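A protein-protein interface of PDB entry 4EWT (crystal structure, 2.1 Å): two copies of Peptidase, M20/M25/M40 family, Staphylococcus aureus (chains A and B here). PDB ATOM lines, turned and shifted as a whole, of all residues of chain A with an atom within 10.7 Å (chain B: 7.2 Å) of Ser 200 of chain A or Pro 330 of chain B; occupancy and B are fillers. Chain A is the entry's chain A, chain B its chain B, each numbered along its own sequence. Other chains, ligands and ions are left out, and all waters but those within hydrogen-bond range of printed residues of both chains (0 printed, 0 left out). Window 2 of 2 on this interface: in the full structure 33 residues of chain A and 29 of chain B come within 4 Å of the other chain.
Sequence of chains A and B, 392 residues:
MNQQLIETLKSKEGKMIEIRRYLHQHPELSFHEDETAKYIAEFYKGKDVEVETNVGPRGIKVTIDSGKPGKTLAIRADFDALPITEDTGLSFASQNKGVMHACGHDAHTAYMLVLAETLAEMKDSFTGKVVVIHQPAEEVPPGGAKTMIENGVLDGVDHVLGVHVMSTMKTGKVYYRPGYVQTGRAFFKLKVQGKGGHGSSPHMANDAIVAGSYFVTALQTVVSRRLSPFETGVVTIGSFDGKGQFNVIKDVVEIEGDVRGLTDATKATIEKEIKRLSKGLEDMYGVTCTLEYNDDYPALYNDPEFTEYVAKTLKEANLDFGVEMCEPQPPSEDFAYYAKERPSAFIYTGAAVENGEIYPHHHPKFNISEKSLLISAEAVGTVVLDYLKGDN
The backbone carbonyl oxygen (O) of Gly 199 of chain A sits at hydrogen-bond distance from the side-chain hydroxyl (OG1) of Thr 236 of chain B.
N of Ile 249 of chain A lies within hydrogen-bond range of O of Gly 197 of chain A, 2.8 Å away.
A ring nitrogen (ND1) of His 198 of chain A lies within hydrogen-bond range of the side-chain hydroxyl (OG) of Ser 200 of chain A (2.9 Å).
The backbone carbonyl oxygen (O) of Asn 247 of chain A sits at hydrogen-bond distance from the backbone NH (N) of Gly 199 of chain A, at 2.9 Å.
The backbone carbonyl oxygen (O) of Val 234 of chain B sits at hydrogen-bond distance from the backbone NH (N) of Arg 260 of chain B (2.9 Å).
The backbone NH of Thr 236 of chain B sits at hydrogen-bond distance from the backbone carbonyl oxygen of Asp 258 of chain B (2.9 Å).
OD1 of Asp 258 of chain B lies within salt-bridge range of NH1 of Arg 260 of chain B, at 3.0 Å.
His 198 of chain A touches Arg 260 of chain B.
O of Gly 199 of chain A touches CG1 of Val 234 of chain B, 3.4 Å away.
OD1 of Asp 258 of chain B touches CA of Gly 199 of chain A, 3.8 Å away.
CB of Ser 200 of chain A touches NE of Arg 260 of chain B, at 3.7 Å.
Pro 330 of chain B touches Ser 200 of chain A.
Asp 258 of chain B touches Phe 246 of chain A (CB to O, 3.0 Å).
Asn 247 of chain A touches Asp 258 of chain B.
CG2 of Thr 236 of chain B touches CG1 of Ile 249 of chain A, at 3.8 Å.
Of chain B, only Val 234, Thr 236 and Asp 258 come within 4 Å of Gly 199 of chain A.
Ser 200 of chain A touches two residues of chain B.
Gln 245 of chain A touches none of the printed residues of chain B.
Printed residues of chain B within 4 Å of Phe 246 of chain A: Asp 258.
Printed residues of chain B within 4 Å of Asn 247 of chain A: Asp 258.
No residue of chain A comes within 4 Å of Thr 183 of chain B.
Of the printed residues of chain A, Thr 236 of chain B touches Gly 199 (3.4 Å) and Ile 249 (3.8 Å).
Printed residues of chain A within 4 Å of Asp 258 of chain B: Gly 199 (3.8 Å), Phe 246 (3.0 Å) and Asn 247 (3.3 Å).
Gln 329 of chain B touches none of the printed residues of chain A.
No residue of chain A comes within 4 Å of Pro 331 of chain B.
No residue of chain A comes within 4 Å of Ser 332 of chain B.
The nearest residue of chain B that does not touch Ser 200 of chain A is Val 234 of chain B (4.5 Å).
The nearest residue of chain A that does not touch Pro 330 of chain B is Ser 201 of chain A (4.2 Å).
Hydrophobic or aromatic side chains of chain A within 4 Å of the printed part of chain B: His 198 and Ile 249.
Of the 16 printed residues of chain B, 5 touch a printed residue of chain A.
Hydrophobic or aromatic side chains of chain B within 4 Å of the printed part of chain A: Val 234.
Among the printed residues, no Asp or Glu carboxylate lies within 4 Å of a Lys or Arg side-chain nitrogen of the other chain.
No position is printed for both chains.
Of the 9 pairs that touch across the chains among the printed residues, none has its exchanged pair printed and touching as well.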
ATOM      1  N   GLY A 196      11.022  21.479 -32.784  1.00  0.00           N
ATOM      2  CA  GLY A 196      11.860  22.648 -32.982  1.00  0.00           C
ATOM      3  C   GLY A 196      12.282  23.310 -31.689  1.00  0.00           C
ATOM      4  O   GLY A 196      11.697  23.071 -30.635  1.00  0.00           O
ATOM      5  N   GLY A 197      13.315  24.136 -31.763  1.00  0.00           N
ATOM      6  CA  GLY A 197      13.795  24.865 -30.593  1.00  0.00           C
ATOM      7  C   GLY A 197      15.003  25.695 -30.968  1.00  0.00           C
ATOM      8  O   GLY A 197      15.546  25.551 -32.066  1.00  0.00           O
ATOM      9  N   HIS A 198      15.407  26.581 -30.061  1.00  0.00           N
ATOM     10  CA  HIS A 198      16.576  27.424 -30.277  1.00  0.00           C
ATOM     11  C   HIS A 198      17.833  26.571 -30.443  1.00  0.00           C
ATOM     12  O   HIS A 198      18.033  25.594 -29.723  1.00  0.00           O
ATOM     13  CB  HIS A 198      16.729  28.426 -29.132  1.00  0.00           C
ATOM     14  CG  HIS A 198      17.524  29.637 -29.499  1.00  0.00           C
ATOM     15  ND1 HIS A 198      18.734  29.941 -28.907  1.00  0.00           N
ATOM     16  CD2 HIS A 198      17.298  30.607 -30.419  1.00  0.00           C
ATOM     17  CE1 HIS A 198      19.210  31.055 -29.437  1.00  0.00           C
ATOM     18  NE2 HIS A 198      18.359  31.478 -30.356  1.00  0.00           N
ATOM     19  N   GLY A 199      18.674  26.952 -31.401  1.00  0.00           N
ATOM     20  CA  GLY A 199      19.854  26.168 -31.785  1.00  0.00           C
ATOM     21  C   GLY A 199      20.901  25.946 -30.709  1.00  0.00           C
ATOM     22  O   GLY A 199      21.734  25.047 -30.833  1.00  0.00           O
ATOM     23  N   SER A 200      20.863  26.755 -29.659  1.00  0.00           N
ATOM     24  CA  SER A 200      21.808  26.633 -28.544  1.00  0.00           C
ATOM     25  C   SER A 200      21.377  25.659 -27.425  1.00  0.00           C
ATOM     26  O   SER A 200      22.095  25.485 -26.435  1.00  0.00           O
ATOM     27  CB  SER A 200      22.033  28.002 -27.937  1.00  0.00           C
ATOM     28  OG  SER A 200      20.799  28.530 -27.485  1.00  0.00           O
ATOM     29  N   SER A 201      20.204  25.050 -27.564  1.00  0.00           N
ATOM     30  CA  SER A 201      19.696  24.132 -26.551  1.00  0.00           C
ATOM     31  C   SER A 201      19.158  22.864 -27.201  1.00  0.00           C
ATOM     32  O   SER A 201      17.942  22.612 -27.153  1.00  0.00           O
ATOM     33  CB  SER A 201      18.601  24.811 -25.726  1.00  0.00           C
ATOM     34  OG  SER A 201      19.131  25.940 -25.062  1.00  0.00           O
ATOM     35  N   PRO A 202      20.056  22.070 -27.820  1.00  0.00           N
ATOM     36  CA  PRO A 202      19.611  20.882 -28.555  1.00  0.00           C
ATOM     37  C   PRO A 202      18.920  19.863 -27.657  1.00  0.00           C
ATOM     38  O   PRO A 202      18.082  19.106 -28.120  1.00  0.00           O
ATOM     39  CB  PRO A 202      20.921  20.301 -29.126  1.00  0.00           C
ATOM     40  CG  PRO A 202      21.993  20.820 -28.216  1.00  0.00           C
ATOM     41  CD  PRO A 202      21.531  22.159 -27.749  1.00  0.00           C
ATOM     42  N   HIS A 203      19.268  19.860 -26.373  1.00  0.00           N
ATOM     43  CA  HIS A 203      18.675  18.926 -25.406  1.00  0.00           C
ATOM     44  C   HIS A 203      17.193  19.169 -25.169  1.00  0.00           C
ATOM     45  O   HIS A 203      16.479  18.269 -24.739  1.00  0.00           O
ATOM     46  CB  HIS A 203      19.407  19.025 -24.070  1.00  0.00           C
ATOM     47  CG  HIS A 203      19.405  20.405 -23.496  1.00  0.00           C
ATOM     48  ND1 HIS A 203      18.886  20.698 -22.249  1.00  0.00           N
ATOM     49  CD2 HIS A 203      19.841  21.578 -24.008  1.00  0.00           C
ATOM     50  CE1 HIS A 203      19.027  21.990 -22.013  1.00  0.00           C
ATOM     51  NE2 HIS A 203      19.603  22.545 -23.065  1.00  0.00           N
ATOM     52  N   MET A 204      16.750  20.371 -25.466  1.00  0.00           N
ATOM     53  CA  MET A 204      15.369  20.802 -25.371  1.00  0.00           C
ATOM     54  C   MET A 204      14.612  20.520 -26.656  1.00  0.00           C
ATOM     55  O   MET A 204      13.458  20.704 -26.730  1.00  0.00           O
ATOM     56  CB  MET A 204      15.272  22.313 -25.167  1.00  0.00           C
ATOM     57  CG  MET A 204      15.510  22.913 -23.811  1.00  0.00           C
ATOM     58  SD  MET A 204      15.507  21.743 -22.549  1.00  0.00           S
ATOM     59  CE  MET A 204      13.800  21.753 -22.040  1.00  0.00           C
ATOM     60  N   ALA A 205      15.309  20.135 -27.691  1.00  0.00           N
ATOM     61  CA  ALA A 205      14.642  19.943 -28.971  1.00  0.00           C
ATOM     62  C   ALA A 205      14.760  18.488 -29.437  1.00  0.00           C
ATOM     63  O   ALA A 205      15.404  17.661 -28.764  1.00  0.00           O
ATOM     64  CB  ALA A 205      15.206  20.921 -30.003  1.00  0.00           C
ATOM     65  N   ASP A 207      15.771  16.957 -33.134  1.00  0.00           N
ATOM     66  CA  ASP A 207      16.247  17.420 -34.434  1.00  0.00           C
ATOM     67  C   ASP A 207      15.690  16.548 -35.576  1.00  0.00           C
ATOM     68  O   ASP A 207      16.066  15.397 -35.715  1.00  0.00           O
ATOM     69  CB  ASP A 207      17.789  17.388 -34.365  1.00  0.00           C
ATOM     70  CG  ASP A 207      18.461  18.194 -35.441  1.00  0.00           C
ATOM     71  OD1 ASP A 207      17.911  18.301 -36.570  1.00  0.00           O
ATOM     72  OD2 ASP A 207      19.580  18.708 -35.156  1.00  0.00           O
ATOM     73  N   GLN A 245      16.048  27.721 -40.819  1.00  0.00           N
ATOM     74  CA  GLN A 245      16.740  28.906 -40.388  1.00  0.00           C
ATOM     75  C   GLN A 245      18.011  28.463 -39.664  1.00  0.00           C
ATOM     76  O   GLN A 245      17.999  27.503 -38.883  1.00  0.00           O
ATOM     77  CB  GLN A 245      15.832  29.731 -39.469  1.00  0.00           C
ATOM     78  CG  GLN A 245      14.349  29.636 -39.849  1.00  0.00           C
ATOM     79  CD  GLN A 245      13.492  30.750 -39.270  1.00  0.00           C
ATOM     80  OE1 GLN A 245      13.856  31.393 -38.281  1.00  0.00           O
ATOM     81  NE2 GLN A 245      12.338  30.992 -39.897  1.00  0.00           N
ATOM     82  N   PHE A 246      19.107  29.170 -39.936  1.00  0.00           N
ATOM     83  CA  PHE A 246      20.431  28.839 -39.391  1.00  0.00           C
ATOM     84  C   PHE A 246      20.591  28.218 -38.005  1.00  0.00           C
ATOM     85  O   PHE A 246      21.248  27.157 -37.828  1.00  0.00           O
ATOM     86  CB  PHE A 246      21.274  30.120 -39.284  1.00  0.00           C
ATOM     87  CG  PHE A 246      22.181  30.304 -40.428  1.00  0.00           C
ATOM     88  CD1 PHE A 246      23.274  29.456 -40.588  1.00  0.00           C
ATOM     89  CD2 PHE A 246      21.924  31.276 -41.388  1.00  0.00           C
ATOM     90  CE1 PHE A 246      24.138  29.598 -41.684  1.00  0.00           C
ATOM     91  CE2 PHE A 246      22.780  31.432 -42.493  1.00  0.00           C
ATOM     92  CZ  PHE A 246      23.886  30.590 -42.638  1.00  0.00           C
ATOM     93  N   ASN A 247      19.937  28.903 -37.063  1.00  0.00           N
ATOM     94  CA  ASN A 247      20.098  28.731 -35.626  1.00  0.00           C
ATOM     95  C   ASN A 247      18.812  28.286 -34.929  1.00  0.00           C
ATOM     96  O   ASN A 247      18.589  28.586 -33.745  1.00  0.00           O
ATOM     97  CB  ASN A 247      20.382  30.112 -35.098  1.00  0.00           C
ATOM     98  CG  ASN A 247      19.555  31.138 -35.805  1.00  0.00           C
ATOM     99  OD1 ASN A 247      18.718  30.787 -36.658  1.00  0.00           O
ATOM    100  ND2 ASN A 247      19.799  32.411 -35.510  1.00  0.00           N
ATOM    101  N   VAL A 248      17.949  27.626 -35.687  1.00  0.00           N
ATOM    102  CA  VAL A 248      16.745  27.025 -35.140  1.00  0.00           C
ATOM    103  C   VAL A 248      16.871  25.550 -35.462  1.00  0.00           C
ATOM    104  O   VAL A 248      17.123  25.186 -36.611  1.00  0.00           O
ATOM    105  CB  VAL A 248      15.466  27.633 -35.789  1.00  0.00           C
ATOM    106  CG1 VAL A 248      14.204  26.891 -35.366  1.00  0.00           C
ATOM    107  CG2 VAL A 248      15.338  29.133 -35.440  1.00  0.00           C
ATOM    108  N   ILE A 249      16.757  24.703 -34.449  1.00  0.00           N
ATOM    109  CA  ILE A 249      16.693  23.257 -34.680  1.00  0.00           C
ATOM    110  C   ILE A 249      15.391  22.915 -35.405  1.00  0.00           C
ATOM    111  O   ILE A 249      14.301  23.272 -34.950  1.00  0.00           O
ATOM    112  CB  ILE A 249      16.838  22.458 -33.364  1.00  0.00           C
ATOM    113  CG1 ILE A 249      18.283  22.539 -32.871  1.00  0.00           C
ATOM    114  CG2 ILE A 249      16.426  20.981 -33.570  1.00  0.00           C
ATOM    115  CD1 ILE A 249      18.429  22.396 -31.375  1.00  0.00           C
ATOM    116  N   LYS A 250      15.523  22.243 -36.543  1.00  0.00           N
ATOM    117  CA  LYS A 250      14.412  22.023 -37.457  1.00  0.00           C
ATOM    118  C   LYS A 250      13.378  21.005 -36.935  1.00  0.00           C
ATOM    119  O   LYS A 250      13.728  19.892 -36.534  1.00  0.00           O
ATOM    120  CB  LYS A 250      14.960  21.644 -38.843  1.00  0.00           C
ATOM    121  CG  LYS A 250      13.916  21.440 -39.939  1.00  0.00           C
ATOM    122  CD  LYS A 250      13.476  22.765 -40.552  1.00  0.00           C
ATOM    123  CE  LYS A 250      12.159  22.630 -41.304  1.00  0.00           C
ATOM    124  NZ  LYS A 250      11.612  23.951 -41.731  1.00  0.00           N
ATOM    125  N   MET B 166      17.638  39.131 -16.513  1.00  0.00           N
ATOM    126  CA  MET B 166      17.246  37.765 -16.786  1.00  0.00           C
ATOM    127  C   MET B 166      15.842  37.420 -16.301  1.00  0.00           C
ATOM    128  O   MET B 166      15.644  37.062 -15.172  1.00  0.00           O
ATOM    129  CB  MET B 166      18.237  36.845 -16.122  1.00  0.00           C
ATOM    130  CG  MET B 166      19.645  37.029 -16.628  1.00  0.00           C
ATOM    131  SD  MET B 166      19.858  36.693 -18.380  1.00  0.00           S
ATOM    132  CE  MET B 166      21.048  35.416 -18.195  1.00  0.00           C
ATOM    133  N   VAL B 181      31.713  32.633 -19.695  1.00  0.00           N
ATOM    134  CA  VAL B 181      30.349  32.586 -19.167  1.00  0.00           C
ATOM    135  C   VAL B 181      29.267  32.465 -20.247  1.00  0.00           C
ATOM    136  O   VAL B 181      28.180  31.949 -19.983  1.00  0.00           O
ATOM    137  CB  VAL B 181      30.059  33.803 -18.214  1.00  0.00           C
ATOM    138  CG1 VAL B 181      30.105  35.137 -18.964  1.00  0.00           C
ATOM    139  CG2 VAL B 181      28.741  33.632 -17.485  1.00  0.00           C
ATOM    140  N   GLN B 182      29.551  32.944 -21.456  1.00  0.00           N
ATOM    141  CA  GLN B 182      28.618  32.763 -22.569  1.00  0.00           C
ATOM    142  C   GLN B 182      29.339  32.348 -23.840  1.00  0.00           C
ATOM    143  O   GLN B 182      30.459  32.775 -24.102  1.00  0.00           O
ATOM    144  CB  GLN B 182      27.726  33.997 -22.786  1.00  0.00           C
ATOM    145  CG  GLN B 182      26.582  34.050 -21.778  1.00  0.00           C
ATOM    146  CD  GLN B 182      25.653  35.253 -21.907  1.00  0.00           C
ATOM    147  OE1 GLN B 182      25.459  35.977 -20.949  1.00  0.00           O
ATOM    148  NE2 GLN B 182      25.053  35.439 -23.072  1.00  0.00           N
ATOM    149  N   THR B 183      28.683  31.477 -24.596  1.00  0.00           N
ATOM    150  CA  THR B 183      29.256  30.885 -25.791  1.00  0.00           C
ATOM    151  C   THR B 183      29.465  31.909 -26.889  1.00  0.00           C
ATOM    152  O   THR B 183      28.701  32.860 -27.014  1.00  0.00           O
ATOM    153  CB  THR B 183      28.356  29.773 -26.345  1.00  0.00           C
ATOM    154  OG1 THR B 183      27.070  30.318 -26.656  1.00  0.00           O
ATOM    155  CG2 THR B 183      28.205  28.650 -25.333  1.00  0.00           C
ATOM    156  N   VAL B 234      28.416  23.147 -29.578  1.00  0.00           N
ATOM    157  CA  VAL B 234      27.179  22.846 -30.263  1.00  0.00           C
ATOM    158  C   VAL B 234      27.461  22.952 -31.763  1.00  0.00           C
ATOM    159  O   VAL B 234      28.074  23.943 -32.224  1.00  0.00           O
ATOM    160  CB  VAL B 234      26.041  23.842 -29.909  1.00  0.00           C
ATOM    161  CG1 VAL B 234      24.704  23.338 -30.445  1.00  0.00           C
ATOM    162  CG2 VAL B 234      25.924  24.053 -28.400  1.00  0.00           C
ATOM    163  N   THR B 236      24.829  22.513 -34.841  1.00  0.00           N
ATOM    164  CA  THR B 236      23.461  22.286 -35.338  1.00  0.00           C
ATOM    165  C   THR B 236      23.364  22.524 -36.845  1.00  0.00           C
ATOM    166  O   THR B 236      23.856  23.538 -37.355  1.00  0.00           O
ATOM    167  CB  THR B 236      22.472  23.221 -34.624  1.00  0.00           C
ATOM    168  OG1 THR B 236      22.304  22.770 -33.277  1.00  0.00           O
ATOM    169  CG2 THR B 236      21.114  23.227 -35.328  1.00  0.00           C
ATOM    170  N   ASP B 258      25.119  26.131 -37.638  1.00  0.00           N
ATOM    171  CA  ASP B 258      25.161  27.088 -36.552  1.00  0.00           C
ATOM    172  C   ASP B 258      26.030  26.401 -35.499  1.00  0.00           C
ATOM    173  O   ASP B 258      25.756  25.244 -35.122  1.00  0.00           O
ATOM    174  CB  ASP B 258      23.703  27.271 -36.087  1.00  0.00           C
ATOM    175  CG  ASP B 258      23.575  27.937 -34.752  1.00  0.00           C
ATOM    176  OD1 ASP B 258      22.698  27.499 -33.960  1.00  0.00           O
ATOM    177  OD2 ASP B 258      24.315  28.910 -34.493  1.00  0.00           O
ATOM    178  N   ARG B 260      28.296  26.745 -31.734  1.00  0.00           N
ATOM    179  CA  ARG B 260      28.628  27.448 -30.485  1.00  0.00           C
ATOM    180  C   ARG B 260      29.825  26.796 -29.808  1.00  0.00           C
ATOM    181  O   ARG B 260      29.973  25.591 -29.838  1.00  0.00           O
ATOM    182  CB  ARG B 260      27.470  27.481 -29.487  1.00  0.00           C
ATOM    183  CG  ARG B 260      26.104  27.902 -30.029  1.00  0.00           C
ATOM    184  CD  ARG B 260      25.904  29.394 -30.088  1.00  0.00           C
ATOM    185  NE  ARG B 260      24.474  29.739 -30.056  1.00  0.00           N
ATOM    186  CZ  ARG B 260      23.690  29.808 -31.133  1.00  0.00           C
ATOM    187  NH1 ARG B 260      24.191  29.559 -32.331  1.00  0.00           N
ATOM    188  NH2 ARG B 260      22.407  30.131 -31.017  1.00  0.00           N
ATOM    189  N   GLU B 327      25.139  29.418 -13.117  1.00  0.00           N
ATOM    190  CA  GLU B 327      25.618  28.588 -14.230  1.00  0.00           C
ATOM    191  C   GLU B 327      25.880  29.461 -15.469  1.00  0.00           C
ATOM    192  O   GLU B 327      25.294  30.547 -15.591  1.00  0.00           O
ATOM    193  CB  GLU B 327      24.605  27.481 -14.549  1.00  0.00           C
ATOM    194  N   PRO B 328      26.771  29.007 -16.385  1.00  0.00           N
ATOM    195  CA  PRO B 328      26.955  29.724 -17.653  1.00  0.00           C
ATOM    196  C   PRO B 328      25.634  29.750 -18.419  1.00  0.00           C
ATOM    197  O   PRO B 328      24.766  28.908 -18.171  1.00  0.00           O
ATOM    198  CB  PRO B 328      27.985  28.871 -18.393  1.00  0.00           C
ATOM    199  CG  PRO B 328      28.708  28.125 -17.327  1.00  0.00           C
ATOM    200  CD  PRO B 328      27.672  27.842 -16.287  1.00  0.00           C
ATOM    201  N   GLN B 329      25.470  30.701 -19.330  1.00  0.00           N
ATOM    202  CA  GLN B 329      24.161  30.903 -19.951  1.00  0.00           C
ATOM    203  C   GLN B 329      24.173  30.650 -21.450  1.00  0.00           C
ATOM    204  O   GLN B 329      25.155  30.957 -22.109  1.00  0.00           O
ATOM    205  CB  GLN B 329      23.628  32.308 -19.637  1.00  0.00           C
ATOM    206  CG  GLN B 329      23.341  32.545 -18.154  1.00  0.00           C
ATOM    207  CD  GLN B 329      22.132  31.771 -17.633  1.00  0.00           C
ATOM    208  OE1 GLN B 329      21.010  31.951 -18.110  1.00  0.00           O
ATOM    209  NE2 GLN B 329      22.359  30.921 -16.635  1.00  0.00           N
ATOM    210  N   PRO B 330      23.075  30.080 -21.990  1.00  0.00           N
ATOM    211  CA  PRO B 330      22.963  29.709 -23.419  1.00  0.00           C
ATOM    212  C   PRO B 330      23.061  30.818 -24.497  1.00  0.00           C
ATOM    213  O   PRO B 330      23.694  30.581 -25.535  1.00  0.00           O
ATOM    214  CB  PRO B 330      21.610  28.977 -23.509  1.00  0.00           C
ATOM    215  CG  PRO B 330      20.918  29.214 -22.179  1.00  0.00           C
ATOM    216  CD  PRO B 330      21.996  29.479 -21.179  1.00  0.00           C
ATOM    217  N   PRO B 331      22.449  32.007 -24.278  1.00  0.00           N
ATOM    218  CA  PRO B 331      22.536  32.997 -25.366  1.00  0.00           C
ATOM    219  C   PRO B 331      23.962  33.447 -25.645  1.00  0.00           C
ATOM    220  O   PRO B 331      24.814  33.399 -24.759  1.00  0.00           O
ATOM    221  CB  PRO B 331      21.748  34.189 -24.816  1.00  0.00           C
ATOM    222  CG  PRO B 331      21.841  34.045 -23.336  1.00  0.00           C
ATOM    223  CD  PRO B 331      21.756  32.571 -23.106  1.00  0.00           C
ATOM    224  N   SER B 332      24.219  33.862 -26.876  1.00  0.00           N
ATOM    225  CA  SER B 332      25.456  34.553 -27.178  1.00  0.00           C
ATOM    226  C   SER B 332      25.141  36.020 -26.959  1.00  0.00           C
ATOM    227  O   SER B 332      23.980  36.422 -27.016  1.00  0.00           O
ATOM    228  CB  SER B 332      25.925  34.266 -28.603  1.00  0.00           C
ATOM    229  OG  SER B 332      26.246  32.892 -28.741  1.00  0.00           O
ATOM    230  N   GLU B 333      26.172  36.802 -26.657  1.00  0.00           N
ATOM    231  CA  GLU B 333      26.006  38.177 -26.223  1.00  0.00           C
ATOM    232  C   GLU B 333      27.159  38.967 -26.807  1.00  0.00           C
ATOM    233  O   GLU B 333      28.315  38.634 -26.564  1.00  0.00           O
ATOM    234  CB  GLU B 333      26.004  38.225 -24.682  1.00  0.00           C
ATOM    235  CG  GLU B 333      26.198  39.599 -24.045  1.00  0.00           C
ATOM    236  CD  GLU B 333      25.108  40.593 -24.395  1.00  0.00           C
ATOM    237  OE1 GLU B 333      23.928  40.331 -24.047  1.00  0.00           O
ATOM    238  OE2 GLU B 333      25.434  41.635 -25.006  1.00  0.00           O
ATOM    239  N   TYR B 348      24.441  39.409 -14.090  1.00  0.00           N
ATOM    240  CA  TYR B 348      23.006  39.297 -14.356  1.00  0.00           C
ATOM    241  C   TYR B 348      22.137  39.798 -13.213  1.00  0.00           C
ATOM    242  O   TYR B 348      22.501  39.679 -12.043  1.00  0.00           O
ATOM    243  CB  TYR B 348      22.639  37.847 -14.670  1.00  0.00           C
ATOM    244  CG  TYR B 348      23.540  37.201 -15.693  1.00  0.00           C
ATOM    245  CD1 TYR B 348      23.518  37.610 -17.025  1.00  0.00           C
ATOM    246  CD2 TYR B 348      24.425  36.185 -15.328  1.00  0.00           C
ATOM    247  CE1 TYR B 348      24.346  37.021 -17.971  1.00  0.00           C
ATOM    248  CE2 TYR B 348      25.257  35.584 -16.271  1.00  0.00           C
ATOM    249  CZ  TYR B 348      25.214  36.012 -17.587  1.00  0.00           C
ATOM    250  OH  TYR B 348      26.033  35.425 -18.527  1.00  0.00           O
